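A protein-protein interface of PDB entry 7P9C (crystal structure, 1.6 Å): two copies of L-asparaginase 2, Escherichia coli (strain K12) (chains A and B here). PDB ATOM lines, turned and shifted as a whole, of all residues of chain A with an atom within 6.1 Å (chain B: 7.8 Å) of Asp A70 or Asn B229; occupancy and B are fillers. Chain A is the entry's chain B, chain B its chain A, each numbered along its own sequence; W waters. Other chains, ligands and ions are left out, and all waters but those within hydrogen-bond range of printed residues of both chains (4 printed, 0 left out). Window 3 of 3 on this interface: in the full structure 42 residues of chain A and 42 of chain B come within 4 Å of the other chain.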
ATOM      1  N   GLN A  66     -16.937  18.231   4.984  1.00  0.00           N
ATOM      2  CA  GLN A  66     -16.369  19.000   3.884  1.00  0.00           C
ATOM      3  C   GLN A  66     -16.409  18.209   2.590  1.00  0.00           C
ATOM      4  O   GLN A  66     -16.239  18.792   1.519  1.00  0.00           O
ATOM      5  CB  GLN A  66     -14.921  19.456   4.159  1.00  0.00           C
ATOM      6  CG  GLN A  66     -13.902  18.315   4.187  1.00  0.00           C
ATOM      7  CD  GLN A  66     -13.759  17.697   5.590  1.00  0.00           C
ATOM      8  OE1 GLN A  66     -14.734  17.497   6.322  1.00  0.00           O
ATOM      9  NE2 GLN A  66     -12.523  17.400   5.965  1.00  0.00           N
ATOM     10  N   ASP A  67     -16.623  16.897   2.677  1.00  0.00           N
ATOM     11  CA  ASP A  67     -16.719  16.003   1.525  1.00  0.00           C
ATOM     12  C   ASP A  67     -18.156  15.590   1.230  1.00  0.00           C
ATOM     13  O   ASP A  67     -18.391  14.687   0.409  1.00  0.00           O
ATOM     14  CB  ASP A  67     -15.863  14.751   1.737  1.00  0.00           C
ATOM     15  CG  ASP A  67     -14.367  15.051   1.721  1.00  0.00           C
ATOM     16  OD1 ASP A  67     -13.946  16.055   1.103  1.00  0.00           O
ATOM     17  OD2 ASP A  67     -13.604  14.248   2.313  1.00  0.00           O
ATOM     18  N   MET A  68     -19.127  16.246   1.858  1.00  0.00           N
ATOM     19  CA  MET A  68     -20.529  15.982   1.575  1.00  0.00           C
ATOM     20  C   MET A  68     -20.814  16.105   0.084  1.00  0.00           C
ATOM     21  O   MET A  68     -20.185  16.898  -0.624  1.00  0.00           O
ATOM     22  CB  MET A  68     -21.389  16.964   2.383  1.00  0.00           C
ATOM     23  CG  MET A  68     -22.853  16.715   2.327  1.00  0.00           C
ATOM     24  SD  MET A  68     -23.382  15.071   2.889  1.00  0.00           S
ATOM     25  CE  MET A  68     -22.414  14.827   4.356  1.00  0.00           C
ATOM     26  N   ASN A  69     -21.805  15.345  -0.385  1.00  0.00           N
ATOM     27  CA  ASN A  69     -22.031  15.253  -1.821  1.00  0.00           C
ATOM     28  C   ASN A  69     -23.456  14.796  -2.119  1.00  0.00           C
ATOM     29  O   ASN A  69     -24.197  14.369  -1.226  1.00  0.00           O
ATOM     30  CB  ASN A  69     -21.035  14.273  -2.446  1.00  0.00           C
ATOM     31  CG  ASN A  69     -21.147  12.885  -1.829  1.00  0.00           C
ATOM     32  OD1 ASN A  69     -22.076  12.145  -2.124  1.00  0.00           O
ATOM     33  ND2 ASN A  69     -20.213  12.539  -0.952  1.00  0.00           N
ATOM     34  N   ASP A  70     -23.804  14.849  -3.419  1.00  0.00           N
ATOM     35  CA  ASP A  70     -25.173  14.578  -3.859  1.00  0.00           C
ATOM     36  C   ASP A  70     -25.595  13.153  -3.488  1.00  0.00           C
ATOM     37  O   ASP A  70     -26.772  12.881  -3.219  1.00  0.00           O
ATOM     38  CB  ASP A  70     -25.317  14.676  -5.386  1.00  0.00           C
ATOM     39  CG  ASP A  70     -25.118  16.072  -5.965  1.00  0.00           C
ATOM     40  OD1 ASP A  70     -25.071  17.102  -5.238  1.00  0.00           O
ATOM     41  OD2 ASP A  70     -25.042  16.103  -7.231  1.00  0.00           O
ATOM     42  N   ASN A  71     -24.667  12.198  -3.572  1.00  0.00           N
ATOM     43  CA  ASN A  71     -25.072  10.811  -3.332  1.00  0.00           C
ATOM     44  C   ASN A  71     -25.520  10.578  -1.889  1.00  0.00           C
ATOM     45  O   ASN A  71     -26.460   9.814  -1.634  1.00  0.00           O
ATOM     46  CB  ASN A  71     -23.935   9.861  -3.691  1.00  0.00           C
ATOM     47  CG  ASN A  71     -23.631   9.836  -5.182  1.00  0.00           C
ATOM     48  OD1 ASN A  71     -24.521  10.022  -6.023  1.00  0.00           O
ATOM     49  ND2 ASN A  71     -22.372   9.597  -5.517  1.00  0.00           N
ATOM     50  N   VAL A  72     -24.859  11.224  -0.928  1.00  0.00           N
ATOM     51  CA  VAL A  72     -25.285  11.132   0.464  1.00  0.00           C
ATOM     52  C   VAL A  72     -26.634  11.812   0.662  1.00  0.00           C
ATOM     53  O   VAL A  72     -27.508  11.313   1.386  1.00  0.00           O
ATOM     54  CB  VAL A  72     -24.205  11.756   1.363  1.00  0.00           C
ATOM     55  CG1 VAL A  72     -24.682  11.767   2.802  1.00  0.00           C
ATOM     56  CG2 VAL A  72     -22.887  10.997   1.227  1.00  0.00           C
ATOM     57  N   TRP A  73     -26.818  12.975   0.041  1.00  0.00           N
ATOM     58  CA  TRP A  73     -28.103  13.662   0.119  1.00  0.00           C
ATOM     59  C   TRP A  73     -29.235  12.756  -0.343  1.00  0.00           C
ATOM     60  O   TRP A  73     -30.235  12.598   0.357  1.00  0.00           O
ATOM     61  CB  TRP A  73     -28.067  14.930  -0.713  1.00  0.00           C
ATOM     62  CG  TRP A  73     -27.290  16.004  -0.075  1.00  0.00           C
ATOM     63  CD1 TRP A  73     -26.653  15.964   1.147  1.00  0.00           C
ATOM     64  CD2 TRP A  73     -27.044  17.287  -0.615  1.00  0.00           C
ATOM     65  NE1 TRP A  73     -26.058  17.165   1.406  1.00  0.00           N
ATOM     66  CE2 TRP A  73     -26.278  18.000   0.338  1.00  0.00           C
ATOM     67  CE3 TRP A  73     -27.410  17.924  -1.808  1.00  0.00           C
ATOM     68  CZ2 TRP A  73     -25.854  19.309   0.124  1.00  0.00           C
ATOM     69  CZ3 TRP A  73     -26.975  19.237  -2.014  1.00  0.00           C
ATOM     70  CH2 TRP A  73     -26.210  19.903  -1.054  1.00  0.00           C
ATOM     71  N   LEU A  74     -29.075  12.111  -1.504  1.00  0.00           N
ATOM     72  CA  LEU A  74     -30.121  11.216  -1.994  1.00  0.00           C
ATOM     73  C   LEU A  74     -30.331  10.043  -1.047  1.00  0.00           C
ATOM     74  O   LEU A  74     -31.469   9.664  -0.760  1.00  0.00           O
ATOM     75  CB  LEU A  74     -29.769  10.705  -3.393  1.00  0.00           C
ATOM     76  CG  LEU A  74     -29.852  11.814  -4.450  1.00  0.00           C
ATOM     77  CD1 LEU A  74     -29.196  11.347  -5.761  1.00  0.00           C
ATOM     78  CD2 LEU A  74     -31.319  12.196  -4.719  1.00  0.00           C
ATOM     79  N   THR A  75     -29.250   9.463  -0.538  1.00  0.00           N
ATOM     80  CA  THR A  75     -29.385   8.374   0.430  1.00  0.00           C
ATOM     81  C   THR A  75     -30.178   8.798   1.661  1.00  0.00           C
ATOM     82  O   THR A  75     -31.054   8.061   2.132  1.00  0.00           O
ATOM     83  CB  THR A  75     -28.010   7.869   0.845  1.00  0.00           C
ATOM     84  OG1 THR A  75     -27.300   7.448  -0.324  1.00  0.00           O
ATOM     85  CG2 THR A  75     -28.131   6.728   1.846  1.00  0.00           C
ATOM     86  N   GLU A 101     -26.254  23.119   4.219  1.00  0.00           N
ATOM     87  CA  GLU A 101     -26.641  22.728   2.869  1.00  0.00           C
ATOM     88  C   GLU A 101     -27.494  21.441   2.944  1.00  0.00           C
ATOM     89  O   GLU A 101     -28.493  21.360   2.304  1.00  0.00           O
ATOM     90  CB  GLU A 101     -25.404  22.455   1.979  1.00  0.00           C
ATOM     91  CG  GLU A 101     -24.503  23.676   1.828  1.00  0.00           C
ATOM     92  CD  GLU A 101     -23.214  23.340   1.121  1.00  0.00           C
ATOM     93  OE1 GLU A 101     -23.278  22.806   0.034  1.00  0.00           O
ATOM     94  OE2 GLU A 101     -22.152  23.613   1.649  1.00  0.00           O
ATOM     95  N   PHE A 105     -31.438  20.859   1.747  1.00  0.00           N
ATOM     96  CA  PHE A 105     -31.803  19.787   0.816  1.00  0.00           C
ATOM     97  C   PHE A 105     -32.913  18.920   1.406  1.00  0.00           C
ATOM     98  O   PHE A 105     -33.932  18.641   0.752  1.00  0.00           O
ATOM     99  CB  PHE A 105     -30.587  18.931   0.463  1.00  0.00           C
ATOM    100  CG  PHE A 105     -30.922  17.790  -0.456  1.00  0.00           C
ATOM    101  CD1 PHE A 105     -31.297  16.553   0.038  1.00  0.00           C
ATOM    102  CD2 PHE A 105     -30.926  17.989  -1.822  1.00  0.00           C
ATOM    103  CE1 PHE A 105     -31.649  15.515  -0.844  1.00  0.00           C
ATOM    104  CE2 PHE A 105     -31.246  16.966  -2.688  1.00  0.00           C
ATOM    105  CZ  PHE A 105     -31.631  15.745  -2.209  1.00  0.00           C
ATOM    106  N   GLU A 217     -29.107  10.723  -9.545  1.00  0.00           N
ATOM    107  CA  GLU A 217     -28.179  11.822  -9.614  1.00  0.00           C
ATOM    108  C   GLU A 217     -28.963  13.107  -9.603  1.00  0.00           C
ATOM    109  O   GLU A 217     -30.146  13.069  -9.795  1.00  0.00           O
ATOM    110  CB  GLU A 217     -27.345  11.758 -10.919  1.00  0.00           C
ATOM    111  CG  GLU A 217     -28.130  11.842 -12.219  1.00  0.00           C
ATOM    112  CD  GLU A 217     -27.233  11.830 -13.441  1.00  0.00           C
ATOM    113  OE1 GLU A 217     -26.501  10.856 -13.645  1.00  0.00           O
ATOM    114  OE2 GLU A 217     -27.265  12.798 -14.207  1.00  0.00           O
ATOM    115  N   LEU A 218     -28.260  14.226  -9.407  1.00  0.00           N
ATOM    116  CA  LEU A 218     -28.854  15.551  -9.427  1.00  0.00           C
ATOM    117  C   LEU A 218     -28.216  16.398 -10.517  1.00  0.00           C
ATOM    118  O   LEU A 218     -27.042  16.193 -10.861  1.00  0.00           O
ATOM    119  CB  LEU A 218     -28.687  16.237  -8.070  1.00  0.00           C
ATOM    120  CG  LEU A 218     -29.414  15.595  -6.870  1.00  0.00           C
ATOM    121  CD1 LEU A 218     -28.943  16.328  -5.576  1.00  0.00           C
ATOM    122  CD2 LEU A 218     -30.870  15.715  -6.998  1.00  0.00           C
ATOM    123  N   PRO A 219     -28.961  17.347 -11.079  1.00  0.00           N
ATOM    124  CA  PRO A 219     -28.373  18.254 -12.079  1.00  0.00           C
ATOM    125  C   PRO A 219     -27.105  18.922 -11.570  1.00  0.00           C
ATOM    126  O   PRO A 219     -26.968  19.229 -10.384  1.00  0.00           O
ATOM    127  CB  PRO A 219     -29.480  19.287 -12.320  1.00  0.00           C
ATOM    128  CG  PRO A 219     -30.773  18.546 -12.007  1.00  0.00           C
ATOM    129  CD  PRO A 219     -30.411  17.573 -10.878  1.00  0.00           C
ATOM    130  N   VAL A 221     -24.670  21.750 -10.805  1.00  0.00           N
ATOM    131  CA  VAL A 221     -24.699  23.170 -10.480  1.00  0.00           C
ATOM    132  C   VAL A 221     -23.415  23.546  -9.743  1.00  0.00           C
ATOM    133  O   VAL A 221     -23.074  22.933  -8.723  1.00  0.00           O
ATOM    134  CB  VAL A 221     -25.930  23.546  -9.629  1.00  0.00           C
ATOM    135  CG1 VAL A 221     -25.893  25.043  -9.229  1.00  0.00           C
ATOM    136  CG2 VAL A 221     -27.213  23.242 -10.369  1.00  0.00           C
ATOM    137  N   TYR A 243     -22.414  22.357 -17.555  1.00  0.00           N
ATOM    138  CA  TYR A 243     -23.163  22.422 -16.307  1.00  0.00           C
ATOM    139  C   TYR A 243     -24.598  22.883 -16.566  1.00  0.00           C
ATOM    140  O   TYR A 243     -24.860  23.724 -17.435  1.00  0.00           O
ATOM    141  CB  TYR A 243     -22.451  23.357 -15.316  1.00  0.00           C
ATOM    142  CG  TYR A 243     -21.621  22.566 -14.344  1.00  0.00           C
ATOM    143  CD1 TYR A 243     -20.635  21.697 -14.810  1.00  0.00           C
ATOM    144  CD2 TYR A 243     -21.860  22.626 -12.968  1.00  0.00           C
ATOM    145  CE1 TYR A 243     -19.907  20.924 -13.938  1.00  0.00           C
ATOM    146  CE2 TYR A 243     -21.130  21.867 -12.091  1.00  0.00           C
ATOM    147  CZ  TYR A 243     -20.162  21.017 -12.579  1.00  0.00           C
ATOM    148  OH  TYR A 243     -19.437  20.229 -11.723  1.00  0.00           O
ATOM    149  N   ARG A 310     -27.642  26.985  -4.597  1.00  0.00           N
ATOM    150  CA  ARG A 310     -27.303  25.804  -5.386  1.00  0.00           C
ATOM    151  C   ARG A 310     -28.254  24.657  -5.098  1.00  0.00           C
ATOM    152  O   ARG A 310     -28.670  23.946  -6.021  1.00  0.00           O
ATOM    153  CB  ARG A 310     -25.854  25.358  -5.127  1.00  0.00           C
ATOM    154  CG  ARG A 310     -25.567  23.946  -5.609  1.00  0.00           C
ATOM    155  CD  ARG A 310     -24.106  23.577  -5.551  1.00  0.00           C
ATOM    156  NE  ARG A 310     -23.901  22.223  -6.079  1.00  0.00           N
ATOM    157  CZ  ARG A 310     -24.077  21.105  -5.381  1.00  0.00           C
ATOM    158  NH1 ARG A 310     -24.442  21.133  -4.116  1.00  0.00           N
ATOM    159  NH2 ARG A 310     -23.919  19.922  -5.979  1.00  0.00           N
ATOM    160  N   GLN A 314     -30.495  23.036  -8.113  1.00  0.00           N
ATOM    161  CA  GLN A 314     -30.410  21.642  -8.533  1.00  0.00           C
ATOM    162  C   GLN A 314     -31.791  21.013  -8.567  1.00  0.00           C
ATOM    163  O   GLN A 314     -32.138  20.302  -9.508  1.00  0.00           O
ATOM    164  CB  GLN A 314     -29.560  20.805  -7.574  1.00  0.00           C
ATOM    165  CG  GLN A 314     -28.085  21.004  -7.651  1.00  0.00           C
ATOM    166  CD  GLN A 314     -27.364  19.990  -6.767  1.00  0.00           C
ATOM    167  OE1 GLN A 314     -27.460  20.051  -5.533  1.00  0.00           O
ATOM    168  NE2 GLN A 314     -26.700  19.024  -7.389  1.00  0.00           N
ATOM    169  N   ASN B 226     -15.901  26.696  -2.010  1.00  0.00           N
ATOM    170  CA  ASN B 226     -16.135  25.328  -1.574  1.00  0.00           C
ATOM    171  C   ASN B 226     -17.570  25.170  -1.069  1.00  0.00           C
ATOM    172  O   ASN B 226     -18.156  26.083  -0.476  1.00  0.00           O
ATOM    173  CB  ASN B 226     -15.175  24.886  -0.464  1.00  0.00           C
ATOM    174  CG  ASN B 226     -13.737  24.721  -0.951  1.00  0.00           C
ATOM    175  OD1 ASN B 226     -13.263  23.602  -1.191  1.00  0.00           O
ATOM    176  ND2 ASN B 226     -13.041  25.844  -1.103  1.00  0.00           N
ATOM    177  N   TYR B 227     -18.114  23.977  -1.306  1.00  0.00           N
ATOM    178  CA  TYR B 227     -19.496  23.618  -1.019  1.00  0.00           C
ATOM    179  C   TYR B 227     -19.599  22.106  -1.276  1.00  0.00           C
ATOM    180  O   TYR B 227     -18.659  21.478  -1.771  1.00  0.00           O
ATOM    181  CB  TYR B 227     -20.460  24.453  -1.881  1.00  0.00           C
ATOM    182  CG  TYR B 227     -20.133  24.420  -3.360  1.00  0.00           C
ATOM    183  CD1 TYR B 227     -19.130  25.217  -3.887  1.00  0.00           C
ATOM    184  CD2 TYR B 227     -20.799  23.563  -4.214  1.00  0.00           C
ATOM    185  CE1 TYR B 227     -18.806  25.177  -5.216  1.00  0.00           C
ATOM    186  CE2 TYR B 227     -20.503  23.534  -5.555  1.00  0.00           C
ATOM    187  CZ  TYR B 227     -19.509  24.350  -6.057  1.00  0.00           C
ATOM    188  OH  TYR B 227     -19.157  24.328  -7.395  1.00  0.00           O
ATOM    189  N   ALA B 228     -20.762  21.502  -0.977  1.00  0.00           N
ATOM    190  CA  ALA B 228     -20.963  20.065  -1.198  1.00  0.00           C
ATOM    191  C   ALA B 228     -20.851  19.698  -2.674  1.00  0.00           C
ATOM    192  O   ALA B 228     -21.377  20.407  -3.525  1.00  0.00           O
ATOM    193  CB  ALA B 228     -22.310  19.603  -0.640  1.00  0.00           C
ATOM    194  N   ASN B 229     -20.120  18.667  -3.010  1.00  0.00           N
ATOM    195  CA  ASN B 229     -20.004  18.242  -4.383  1.00  0.00           C
ATOM    196  C   ASN B 229     -19.444  19.386  -5.240  1.00  0.00           C
ATOM    197  O   ASN B 229     -19.831  19.550  -6.348  1.00  0.00           O
ATOM    198  CB  ASN B 229     -21.361  17.852  -4.906  1.00  0.00           C
ATOM    199  CG  ASN B 229     -21.317  16.661  -5.841  1.00  0.00           C
ATOM    200  OD1 ASN B 229     -21.879  15.645  -5.553  1.00  0.00           O
ATOM    201  ND2 ASN B 229     -20.676  16.809  -6.972  1.00  0.00           N
ATOM    202  N   ALA B 230     -18.457  20.081  -4.715  1.00  0.00           N
ATOM    203  CA  ALA B 230     -17.830  21.139  -5.498  1.00  0.00           C
ATOM    204  C   ALA B 230     -16.962  20.618  -6.638  1.00  0.00           C
ATOM    205  O   ALA B 230     -16.182  19.670  -6.481  1.00  0.00           O
ATOM    206  CB  ALA B 230     -16.985  22.025  -4.583  1.00  0.00           C
ATOM    207  N   SER B 231     -17.099  21.259  -7.795  1.00  0.00           N
ATOM    208  CA  SER B 231     -16.297  20.904  -8.961  1.00  0.00           C
ATOM    209  C   SER B 231     -14.862  21.395  -8.790  1.00  0.00           C
ATOM    210  O   SER B 231     -14.625  22.467  -8.232  1.00  0.00           O
ATOM    211  CB  SER B 231     -16.897  21.525 -10.224  1.00  0.00           C
ATOM    212  OG  SER B 231     -16.029  21.406 -11.333  1.00  0.00           O
ATOM    213  N   ASP B 232     -13.906  20.611  -9.268  1.00  0.00           N
ATOM    214  CA  ASP B 232     -12.533  21.092  -9.329  1.00  0.00           C
ATOM    215  C   ASP B 232     -12.262  21.958 -10.558  1.00  0.00           C
ATOM    216  O   ASP B 232     -11.136  22.433 -10.723  1.00  0.00           O
ATOM    217  CB  ASP B 232     -11.531  19.916  -9.288  1.00  0.00           C
ATOM    218  CG  ASP B 232     -11.661  18.955 -10.469  1.00  0.00           C
ATOM    219  OD1 ASP B 232     -12.378  19.237 -11.449  1.00  0.00           O
ATOM    220  OD2 ASP B 232     -11.027  17.878 -10.416  1.00  0.00           O
ATOM    221  N   TYR B 257     -13.337  20.835  -0.111  1.00  0.00           N
ATOM    222  CA  TYR B 257     -13.955  19.677  -0.742  1.00  0.00           C
ATOM    223  C   TYR B 257     -12.857  18.834  -1.394  1.00  0.00           C
ATOM    224  O   TYR B 257     -11.901  19.368  -1.963  1.00  0.00           O
ATOM    225  CB  TYR B 257     -15.009  20.128  -1.781  1.00  0.00           C
ATOM    226  CG  TYR B 257     -15.692  18.934  -2.397  1.00  0.00           C
ATOM    227  CD1 TYR B 257     -16.610  18.205  -1.660  1.00  0.00           C
ATOM    228  CD2 TYR B 257     -15.375  18.500  -3.684  1.00  0.00           C
ATOM    229  CE1 TYR B 257     -17.182  17.072  -2.176  1.00  0.00           C
ATOM    230  CE2 TYR B 257     -15.962  17.372  -4.223  1.00  0.00           C
ATOM    231  CZ  TYR B 257     -16.865  16.667  -3.464  1.00  0.00           C
ATOM    232  OH  TYR B 257     -17.465  15.545  -3.953  1.00  0.00           O
ATOM    233  N   LYS B 258     -13.007  17.508  -1.347  1.00  0.00           N
ATOM    234  CA  LYS B 258     -11.902  16.620  -1.722  1.00  0.00           C
ATOM    235  C   LYS B 258     -11.331  16.928  -3.112  1.00  0.00           C
ATOM    236  O   LYS B 258     -10.109  16.994  -3.284  1.00  0.00           O
ATOM    237  CB  LYS B 258     -12.343  15.162  -1.632  1.00  0.00           C
ATOM    238  CG  LYS B 258     -13.444  14.734  -2.561  1.00  0.00           C
ATOM    239  CD  LYS B 258     -14.184  13.494  -1.986  1.00  0.00           C
ATOM    240  CE  LYS B 258     -15.023  12.794  -3.039  1.00  0.00           C
ATOM    241  NZ  LYS B 258     -15.957  11.789  -2.409  1.00  0.00           N
ATOM    242  N   SER B 259     -12.185  17.156  -4.111  1.00  0.00           N
ATOM    243  CA  SER B 259     -11.665  17.405  -5.461  1.00  0.00           C
ATOM    244  C   SER B 259     -10.875  18.709  -5.531  1.00  0.00           C
ATOM    245  O   SER B 259      -9.886  18.817  -6.276  1.00  0.00           O
ATOM    246  CB  SER B 259     -12.816  17.456  -6.469  1.00  0.00           C
ATOM    247  OG  SER B 259     -13.559  16.254  -6.432  1.00  0.00           O
ATOM    248  N   VAL B 260     -11.349  19.734  -4.821  1.00  0.00           N
ATOM    249  CA  VAL B 260     -10.665  21.020  -4.787  1.00  0.00           C
ATOM    250  C   VAL B 260      -9.339  20.893  -4.048  1.00  0.00           C
ATOM    251  O   VAL B 260      -8.317  21.429  -4.477  1.00  0.00           O
ATOM    252  CB  VAL B 260     -11.589  22.061  -4.128  1.00  0.00           C
ATOM    253  CG1 VAL B 260     -10.887  23.412  -3.994  1.00  0.00           C
ATOM    254  CG2 VAL B 260     -12.905  22.215  -4.924  1.00  0.00           C
HETATM  255  O   HOH W   1     -11.477  17.069   1.692  1.00  0.00           O
HETATM  256  O   HOH W   2     -16.978  21.500   0.798  1.00  0.00           O
HETATM  257  O   HOH W   3     -20.680  19.870  -9.072  1.00  0.00           O
HETATM  258  O   HOH W   4     -22.027  12.850  -5.671  1.00  0.00           O
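No position is printed for both chains.
Of chain B, only Asn B229 (3.0 Å) comes within 4 Å of Asp A70. Printed residues of chain B within 4 Å of Tyr A243: Ser B231 (3.2 Å). Printed residues of chain A within 4 Å of Ala B228: Met A68 (3.3 Å), Trp A73 (3.6 Å), Glu A101 (3.0 Å) and Arg A310 (3.2 Å). Printed residues of chain A within 4 Å of Tyr B257: Gln A66, Asp A67 and Met A68. The nearest residue of chain B that does not touch Asp A70 is Ala B228 (5.2 Å). The nearest residue of chain A that does not touch Asn B229 is Asn A71 (4.9 Å). The nearest printed residue of chain B that does not touch Asp A67 is Asn B229 (5.5 Å).
The side-chain amide oxygen (OD1) of Asn B226 is in hydrogen-bond range of the backbone NH (N) of Tyr B257 (3.0 Å). The side-chain amide oxygen (OD1) of Asn A69 sits at hydrogen-bond distance from the backbone NH (N) of Asn A71, at 3.0 Å. The backbone NH of Val A72 lies within hydrogen-bond range of the side-chain amide oxygen of Asn A69. OD1 of Asp A70 lies within salt-bridge range of NH2 of Arg A310, at 3.1 Å. O of Val A221 is in hydrogen-bond range of NE of Arg A310, 2.9 Å away. NE2 of Gln A314 lies close to NH2 of Arg A310.
Among the printed residues, pairs that only touch across the chains: Tyr A243 with Ser B231 (3.2 Å), Gln A66 with Tyr B257 (3.3 Å), Met A68 with Ala B228 (3.3 Å), Met A68 with Tyr B257 (3.4 Å), Arg A310 with Asn B229 (3.5 Å), Asn A69 with Asn B229 (3.5 Å), Arg A310 with Tyr B227 (3.6 Å), Trp A73 with Ala B228 (3.6 Å), Asp A67 with Tyr B257 (3.7 Å) and Glu A101 with Tyr B227 (3.8 Å).
Along chain A the printed residues that touch a printed residue of chain B span positions 66 to 310. Printed residues of chain B that touch a printed residue of chain A: Tyr B227, Ala B228, Asn B229, Ser B231, Tyr B257 and Lys B258.
Water W1 bridges OD1 of Asp A67 (2.7 Å) and N of Lys B258 (3.4 Å). Water W4 lies within hydrogen-bond range of the side-chain amide oxygen of Asn B229, the side-chain amide nitrogen of Asn A71 and the backbone NH of Asp A70. Water W3 lies within hydrogen-bond range of the backbone carbonyl oxygen of Asn B229 (2.9 Å) and the side-chain hydroxyl of Tyr A243 (2.9 Å). Water W2 lies within hydrogen-bond range of O of Gln A66 and O of Tyr B227.
OE1 of Glu A101 is in hydrogen-bond range of N of Ala B228, at 3.0 Å. O of Ala B228 lies within hydrogen-bond range of NH1 of Arg A310. The backbone carbonyl oxygen (O) of Met A68 is in hydrogen-bond range of the backbone NH (N) of Asn B229 (3.0 Å). The backbone NH (N) of Asp A70 lies within hydrogen-bond range of the side-chain amide oxygen (OD1) of Asn B229. OD1 of Asp A67 is in hydrogen-bond range of N of Lys B258 (3.0 Å).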
